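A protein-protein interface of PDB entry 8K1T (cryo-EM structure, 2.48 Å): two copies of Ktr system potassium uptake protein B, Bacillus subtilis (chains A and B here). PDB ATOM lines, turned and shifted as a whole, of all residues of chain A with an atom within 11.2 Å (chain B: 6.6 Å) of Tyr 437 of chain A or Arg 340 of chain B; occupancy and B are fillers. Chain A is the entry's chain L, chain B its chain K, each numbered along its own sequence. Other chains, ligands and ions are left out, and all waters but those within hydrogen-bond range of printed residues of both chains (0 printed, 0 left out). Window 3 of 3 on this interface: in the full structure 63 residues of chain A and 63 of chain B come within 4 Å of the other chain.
Among the printed residues, pairs that only touch across the chains: Pro 438 of chain A with Arg 341 of chain B, Tyr 437 of chain A with Glu 335 of chain B, Tyr 437 of chain A with Arg 340 of chain B, Tyr 437 of chain A with Val 337 of chain B, Gly 440 of chain A with Leu 226 of chain B, Asp 439 of chain A with Arg 341 of chain B, Glu 441 of chain A with Leu 226 of chain B and Gly 440 of chain A with Arg 341 of chain B.
No position is printed for both chains.
Of the 11 printed residues of chain A, 7 touch a printed residue of chain B. Hydrophobic or aromatic side chains of chain A that line the printed part of chain B: Tyr 437 and Pro 438. Among the printed residues, 14 pairs touch across the chains. Among the printed residues, Asp or Glu carboxylates within 4 Å of a Lys or Arg side-chain nitrogen of the other chain: Arg 436 of chain A with Glu 335 of chain B (3.8 Å).
The side-chain carboxylate (OE2) of Glu 335 of chain B lies within salt-bridge range of the guanidinium group (NH1) of Arg 436 of chain A. The side-chain hydroxyl of Ser 342 of chain B lies within hydrogen-bond range of the backbone carbonyl oxygen of Tyr 437 of chain A. O of Pro 438 of chain A lies within hydrogen-bond range of N of Ser 342 of chain B (2.9 Å). The side-chain hydroxyl (OG) of Ser 342 of chain B sits at hydrogen-bond distance from the side-chain carboxylate (OD1) of Asp 439 of chain A (3.1 Å). N of Gly 440 of chain A is in hydrogen-bond range of O of Ser 342 of chain B (2.8 Å). The backbone carbonyl oxygen of Ile 435 of chain A sits close to the side-chain carboxylate of Glu 335 of chain B, 3.0 Å away.
Tyr 437 of chain A touches just these residues of chain B: Glu 335 (3.3 Å), Val 337 (3.5 Å), Arg 340 (3.5 Å) and Ser 342 (3.2 Å). Printed residues of chain B within 4 Å of Pro 438 of chain A: Arg 341 (3.3 Å) and Ser 342 (2.9 Å). Printed residues of chain B within 4 Å of Gly 440 of chain A: Leu 226, Arg 341 and Ser 342. Arg 340 of chain B touches one residue of chain A. Ser 342 of chain B touches four residues of chain A. Ile 343 of chain B touches none of the printed residues of chain A. The nearest printed residue of chain B that does not touch Pro 438 of chain A is Arg 340 of chain B (4.1 Å).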
ATOM      1  N   GLU A 431      -4.021  17.042  17.652  1.00  0.00           N
ATOM      2  CA  GLU A 431      -3.745  18.195  18.496  1.00  0.00           C
ATOM      3  C   GLU A 431      -4.941  18.411  19.410  1.00  0.00           C
ATOM      4  O   GLU A 431      -6.089  18.366  18.958  1.00  0.00           O
ATOM      5  CB  GLU A 431      -3.456  19.448  17.663  1.00  0.00           C
ATOM      6  CG  GLU A 431      -4.557  19.853  16.687  1.00  0.00           C
ATOM      7  CD  GLU A 431      -4.599  18.982  15.443  1.00  0.00           C
ATOM      8  OE1 GLU A 431      -3.649  18.200  15.230  1.00  0.00           O
ATOM      9  OE2 GLU A 431      -5.585  19.077  14.682  1.00  0.00           O
ATOM     10  N   GLN A 432      -4.672  18.624  20.693  1.00  0.00           N
ATOM     11  CA  GLN A 432      -5.734  18.767  21.676  1.00  0.00           C
ATOM     12  C   GLN A 432      -6.183  20.219  21.766  1.00  0.00           C
ATOM     13  O   GLN A 432      -5.383  21.118  22.040  1.00  0.00           O
ATOM     14  CB  GLN A 432      -5.271  18.272  23.047  1.00  0.00           C
ATOM     15  CG  GLN A 432      -4.957  16.787  23.090  1.00  0.00           C
ATOM     16  CD  GLN A 432      -4.630  16.300  24.487  1.00  0.00           C
ATOM     17  OE1 GLN A 432      -4.752  17.043  25.461  1.00  0.00           O
ATOM     18  NE2 GLN A 432      -4.213  15.044  24.594  1.00  0.00           N
ATOM     19  N   SER A 433      -7.471  20.440  21.526  1.00  0.00           N
ATOM     20  CA  SER A 433      -8.091  21.748  21.671  1.00  0.00           C
ATOM     21  C   SER A 433      -9.198  21.652  22.708  1.00  0.00           C
ATOM     22  O   SER A 433     -10.055  20.767  22.632  1.00  0.00           O
ATOM     23  CB  SER A 433      -8.650  22.252  20.338  1.00  0.00           C
ATOM     24  OG  SER A 433      -7.621  22.382  19.373  1.00  0.00           O
ATOM     25  N   ASN A 434      -9.175  22.562  23.677  1.00  0.00           N
ATOM     26  CA  ASN A 434     -10.152  22.568  24.754  1.00  0.00           C
ATOM     27  C   ASN A 434     -11.371  23.420  24.439  1.00  0.00           C
ATOM     28  O   ASN A 434     -12.276  23.517  25.274  1.00  0.00           O
ATOM     29  CB  ASN A 434      -9.501  23.057  26.050  1.00  0.00           C
ATOM     30  CG  ASN A 434      -8.264  22.266  26.413  1.00  0.00           C
ATOM     31  OD1 ASN A 434      -7.149  22.783  26.372  1.00  0.00           O
ATOM     32  ND2 ASN A 434      -8.454  21.003  26.773  1.00  0.00           N
ATOM     33  N   ILE A 435     -11.423  24.031  23.264  1.00  0.00           N
ATOM     34  CA  ILE A 435     -12.524  24.920  22.921  1.00  0.00           C
ATOM     35  C   ILE A 435     -13.720  24.104  22.451  1.00  0.00           C
ATOM     36  O   ILE A 435     -13.582  23.057  21.811  1.00  0.00           O
ATOM     37  CB  ILE A 435     -12.086  25.948  21.859  1.00  0.00           C
ATOM     38  CG1 ILE A 435     -11.846  25.272  20.513  1.00  0.00           C
ATOM     39  CG2 ILE A 435     -10.834  26.672  22.313  1.00  0.00           C
ATOM     40  CD1 ILE A 435     -11.534  26.238  19.402  1.00  0.00           C
ATOM     41  N   ARG A 436     -14.909  24.585  22.789  1.00  0.00           N
ATOM     42  CA  ARG A 436     -16.162  23.966  22.397  1.00  0.00           C
ATOM     43  C   ARG A 436     -16.929  24.918  21.490  1.00  0.00           C
ATOM     44  O   ARG A 436     -16.535  26.065  21.277  1.00  0.00           O
ATOM     45  CB  ARG A 436     -16.998  23.593  23.625  1.00  0.00           C
ATOM     46  CG  ARG A 436     -16.349  22.553  24.516  1.00  0.00           C
ATOM     47  CD  ARG A 436     -16.319  21.195  23.839  1.00  0.00           C
ATOM     48  NE  ARG A 436     -15.548  20.212  24.590  1.00  0.00           N
ATOM     49  CZ  ARG A 436     -14.310  19.841  24.290  1.00  0.00           C
ATOM     50  NH1 ARG A 436     -13.670  20.345  23.247  1.00  0.00           N
ATOM     51  NH2 ARG A 436     -13.700  18.940  25.054  1.00  0.00           N
ATOM     52  N   TYR A 437     -18.034  24.425  20.945  1.00  0.00           N
ATOM     53  CA  TYR A 437     -18.841  25.197  20.017  1.00  0.00           C
ATOM     54  C   TYR A 437     -20.304  25.127  20.415  1.00  0.00           C
ATOM     55  O   TYR A 437     -20.730  24.172  21.070  1.00  0.00           O
ATOM     56  CB  TYR A 437     -18.671  24.685  18.582  1.00  0.00           C
ATOM     57  CG  TYR A 437     -17.308  24.967  18.005  1.00  0.00           C
ATOM     58  CD1 TYR A 437     -16.259  24.080  18.188  1.00  0.00           C
ATOM     59  CD2 TYR A 437     -17.069  26.123  17.286  1.00  0.00           C
ATOM     60  CE1 TYR A 437     -15.012  24.337  17.664  1.00  0.00           C
ATOM     61  CE2 TYR A 437     -15.828  26.387  16.758  1.00  0.00           C
ATOM     62  CZ  TYR A 437     -14.803  25.493  16.949  1.00  0.00           C
ATOM     63  OH  TYR A 437     -13.563  25.761  16.422  1.00  0.00           O
ATOM     64  N   PRO A 438     -21.093  26.138  20.055  1.00  0.00           N
ATOM     65  CA  PRO A 438     -22.529  26.078  20.332  1.00  0.00           C
ATOM     66  C   PRO A 438     -23.190  24.951  19.555  1.00  0.00           C
ATOM     67  O   PRO A 438     -22.763  24.589  18.457  1.00  0.00           O
ATOM     68  CB  PRO A 438     -23.037  27.451  19.878  1.00  0.00           C
ATOM     69  CG  PRO A 438     -22.019  27.928  18.910  1.00  0.00           C
ATOM     70  CD  PRO A 438     -20.713  27.400  19.399  1.00  0.00           C
ATOM     71  N   ASP A 439     -24.239  24.390  20.145  1.00  0.00           N
ATOM     72  CA  ASP A 439     -24.923  23.258  19.540  1.00  0.00           C
ATOM     73  C   ASP A 439     -25.563  23.651  18.216  1.00  0.00           C
ATOM     74  O   ASP A 439     -26.066  24.765  18.053  1.00  0.00           O
ATOM     75  CB  ASP A 439     -25.987  22.710  20.487  1.00  0.00           C
ATOM     76  CG  ASP A 439     -25.392  22.105  21.738  1.00  0.00           C
ATOM     77  OD1 ASP A 439     -24.152  22.123  21.876  1.00  0.00           O
ATOM     78  OD2 ASP A 439     -26.166  21.609  22.584  1.00  0.00           O
ATOM     79  N   GLY A 440     -25.535  22.725  17.265  1.00  0.00           N
ATOM     80  CA  GLY A 440     -26.205  22.902  15.995  1.00  0.00           C
ATOM     81  C   GLY A 440     -27.261  21.832  15.807  1.00  0.00           C
ATOM     82  O   GLY A 440     -27.110  20.702  16.270  1.00  0.00           O
ATOM     83  N   GLU A 441     -28.340  22.202  15.128  1.00  0.00           N
ATOM     84  CA  GLU A 441     -29.434  21.284  14.856  1.00  0.00           C
ATOM     85  C   GLU A 441     -29.406  20.856  13.395  1.00  0.00           C
ATOM     86  O   GLU A 441     -29.202  21.672  12.494  1.00  0.00           O
ATOM     87  CB  GLU A 441     -30.785  21.919  15.196  1.00  0.00           C
ATOM     88  CG  GLU A 441     -31.050  23.246  14.507  1.00  0.00           C
ATOM     89  CD  GLU A 441     -32.427  23.801  14.820  1.00  0.00           C
ATOM     90  OE1 GLU A 441     -33.151  23.178  15.624  1.00  0.00           O
ATOM     91  OE2 GLU A 441     -32.784  24.859  14.260  1.00  0.00           O
ATOM     92  N   LEU B 226     -27.887  25.564  10.294  1.00  0.00           N
ATOM     93  CA  LEU B 226     -26.843  24.574  10.055  1.00  0.00           C
ATOM     94  C   LEU B 226     -27.311  23.507   9.075  1.00  0.00           C
ATOM     95  O   LEU B 226     -26.552  23.083   8.198  1.00  0.00           O
ATOM     96  CB  LEU B 226     -26.405  23.942  11.374  1.00  0.00           C
ATOM     97  CG  LEU B 226     -25.389  22.808  11.253  1.00  0.00           C
ATOM     98  CD1 LEU B 226     -24.112  23.301  10.600  1.00  0.00           C
ATOM     99  CD2 LEU B 226     -25.101  22.201  12.610  1.00  0.00           C
ATOM    100  N   LYS B 229     -27.276  24.966   5.513  1.00  0.00           N
ATOM    101  CA  LYS B 229     -25.926  25.115   4.984  1.00  0.00           C
ATOM    102  C   LYS B 229     -25.325  23.768   4.606  1.00  0.00           C
ATOM    103  O   LYS B 229     -24.595  23.665   3.614  1.00  0.00           O
ATOM    104  CB  LYS B 229     -25.042  25.836   5.999  1.00  0.00           C
ATOM    105  CG  LYS B 229     -25.436  27.284   6.230  1.00  0.00           C
ATOM    106  CD  LYS B 229     -24.432  28.012   7.105  1.00  0.00           C
ATOM    107  CE  LYS B 229     -24.384  27.422   8.501  1.00  0.00           C
ATOM    108  NZ  LYS B 229     -23.465  28.184   9.389  1.00  0.00           N
ATOM    109  N   GLU B 335     -15.279  16.322  20.005  1.00  0.00           N
ATOM    110  CA  GLU B 335     -16.597  16.774  19.590  1.00  0.00           C
ATOM    111  C   GLU B 335     -16.675  16.789  18.072  1.00  0.00           C
ATOM    112  O   GLU B 335     -15.669  16.979  17.386  1.00  0.00           O
ATOM    113  CB  GLU B 335     -16.913  18.165  20.153  1.00  0.00           C
ATOM    114  CG  GLU B 335     -15.871  19.217  19.812  1.00  0.00           C
ATOM    115  CD  GLU B 335     -16.266  20.609  20.268  1.00  0.00           C
ATOM    116  OE1 GLU B 335     -17.388  20.776  20.789  1.00  0.00           O
ATOM    117  OE2 GLU B 335     -15.449  21.538  20.099  1.00  0.00           O
ATOM    118  N   VAL B 337     -17.819  18.755  14.953  1.00  0.00           N
ATOM    119  CA  VAL B 337     -18.056  20.158  14.636  1.00  0.00           C
ATOM    120  C   VAL B 337     -18.144  20.321  13.127  1.00  0.00           C
ATOM    121  O   VAL B 337     -17.216  19.951  12.402  1.00  0.00           O
ATOM    122  CB  VAL B 337     -16.952  21.065  15.212  1.00  0.00           C
ATOM    123  CG1 VAL B 337     -17.194  22.511  14.822  1.00  0.00           C
ATOM    124  CG2 VAL B 337     -16.888  20.922  16.718  1.00  0.00           C
ATOM    125  N   ILE B 338     -19.261  20.872  12.658  1.00  0.00           N
ATOM    126  CA  ILE B 338     -19.433  21.257  11.261  1.00  0.00           C
ATOM    127  C   ILE B 338     -19.931  22.693  11.235  1.00  0.00           C
ATOM    128  O   ILE B 338     -20.863  23.040  11.965  1.00  0.00           O
ATOM    129  CB  ILE B 338     -20.423  20.346  10.508  1.00  0.00           C
ATOM    130  CG1 ILE B 338     -20.306  18.899  10.974  1.00  0.00           C
ATOM    131  CG2 ILE B 338     -20.176  20.427   9.013  1.00  0.00           C
ATOM    132  CD1 ILE B 338     -21.139  17.939  10.162  1.00  0.00           C
ATOM    133  N   PHE B 339     -19.317  23.522  10.390  1.00  0.00           N
ATOM    134  CA  PHE B 339     -19.696  24.929  10.254  1.00  0.00           C
ATOM    135  C   PHE B 339     -19.689  25.639  11.605  1.00  0.00           C
ATOM    136  O   PHE B 339     -20.580  26.429  11.918  1.00  0.00           O
ATOM    137  CB  PHE B 339     -21.060  25.074   9.580  1.00  0.00           C
ATOM    138  CG  PHE B 339     -21.051  24.772   8.112  1.00  0.00           C
ATOM    139  CD1 PHE B 339     -20.488  25.661   7.214  1.00  0.00           C
ATOM    140  CD2 PHE B 339     -21.623  23.612   7.627  1.00  0.00           C
ATOM    141  CE1 PHE B 339     -20.484  25.388   5.863  1.00  0.00           C
ATOM    142  CE2 PHE B 339     -21.620  23.337   6.277  1.00  0.00           C
ATOM    143  CZ  PHE B 339     -21.050  24.225   5.395  1.00  0.00           C
ATOM    144  N   ARG B 340     -18.673  25.341  12.416  1.00  0.00           N
ATOM    145  CA  ARG B 340     -18.493  25.950  13.732  1.00  0.00           C
ATOM    146  C   ARG B 340     -19.673  25.669  14.658  1.00  0.00           C
ATOM    147  O   ARG B 340     -20.015  26.488  15.510  1.00  0.00           O
ATOM    148  CB  ARG B 340     -18.249  27.455  13.616  1.00  0.00           C
ATOM    149  CG  ARG B 340     -17.035  27.823  12.786  1.00  0.00           C
ATOM    150  CD  ARG B 340     -17.043  29.298  12.438  1.00  0.00           C
ATOM    151  NE  ARG B 340     -15.818  29.707  11.762  1.00  0.00           N
ATOM    152  CZ  ARG B 340     -15.579  30.937  11.329  1.00  0.00           C
ATOM    153  NH1 ARG B 340     -16.463  31.909  11.482  1.00  0.00           N
ATOM    154  NH2 ARG B 340     -14.422  31.199  10.727  1.00  0.00           N
ATOM    155  N   ARG B 341     -20.304  24.510  14.495  1.00  0.00           N
ATOM    156  CA  ARG B 341     -21.391  24.089  15.364  1.00  0.00           C
ATOM    157  C   ARG B 341     -21.119  22.673  15.839  1.00  0.00           C
ATOM    158  O   ARG B 341     -20.801  21.796  15.035  1.00  0.00           O
ATOM    159  CB  ARG B 341     -22.745  24.141  14.648  1.00  0.00           C
ATOM    160  CG  ARG B 341     -23.296  25.534  14.426  1.00  0.00           C
ATOM    161  CD  ARG B 341     -23.551  26.242  15.743  1.00  0.00           C
ATOM    162  NE  ARG B 341     -24.460  27.369  15.589  1.00  0.00           N
ATOM    163  CZ  ARG B 341     -24.098  28.569  15.156  1.00  0.00           C
ATOM    164  NH1 ARG B 341     -22.848  28.834  14.818  1.00  0.00           N
ATOM    165  NH2 ARG B 341     -25.015  29.526  15.058  1.00  0.00           N
ATOM    166  N   SER B 342     -21.239  22.455  17.140  1.00  0.00           N
ATOM    167  CA  SER B 342     -21.074  21.122  17.690  1.00  0.00           C
ATOM    168  C   SER B 342     -22.344  20.308  17.479  1.00  0.00           C
ATOM    169  O   SER B 342     -23.460  20.830  17.507  1.00  0.00           O
ATOM    170  CB  SER B 342     -20.728  21.179  19.177  1.00  0.00           C
ATOM    171  OG  SER B 342     -21.886  21.390  19.960  1.00  0.00           O
ATOM    172  N   ILE B 343     -22.162  19.011  17.260  1.00  0.00           N
ATOM    173  CA  ILE B 343     -23.263  18.088  17.015  1.00  0.00           C
ATOM    174  C   ILE B 343     -23.369  17.158  18.212  1.00  0.00           C
ATOM    175  O   ILE B 343     -22.410  16.448  18.542  1.00  0.00           O
ATOM    176  CB  ILE B 343     -23.067  17.303  15.711  1.00  0.00           C
ATOM    177  CG1 ILE B 343     -23.049  18.266  14.525  1.00  0.00           C
ATOM    178  CG2 ILE B 343     -24.165  16.277  15.540  1.00  0.00           C
ATOM    179  CD1 ILE B 343     -23.003  17.580  13.193  1.00  0.00           C
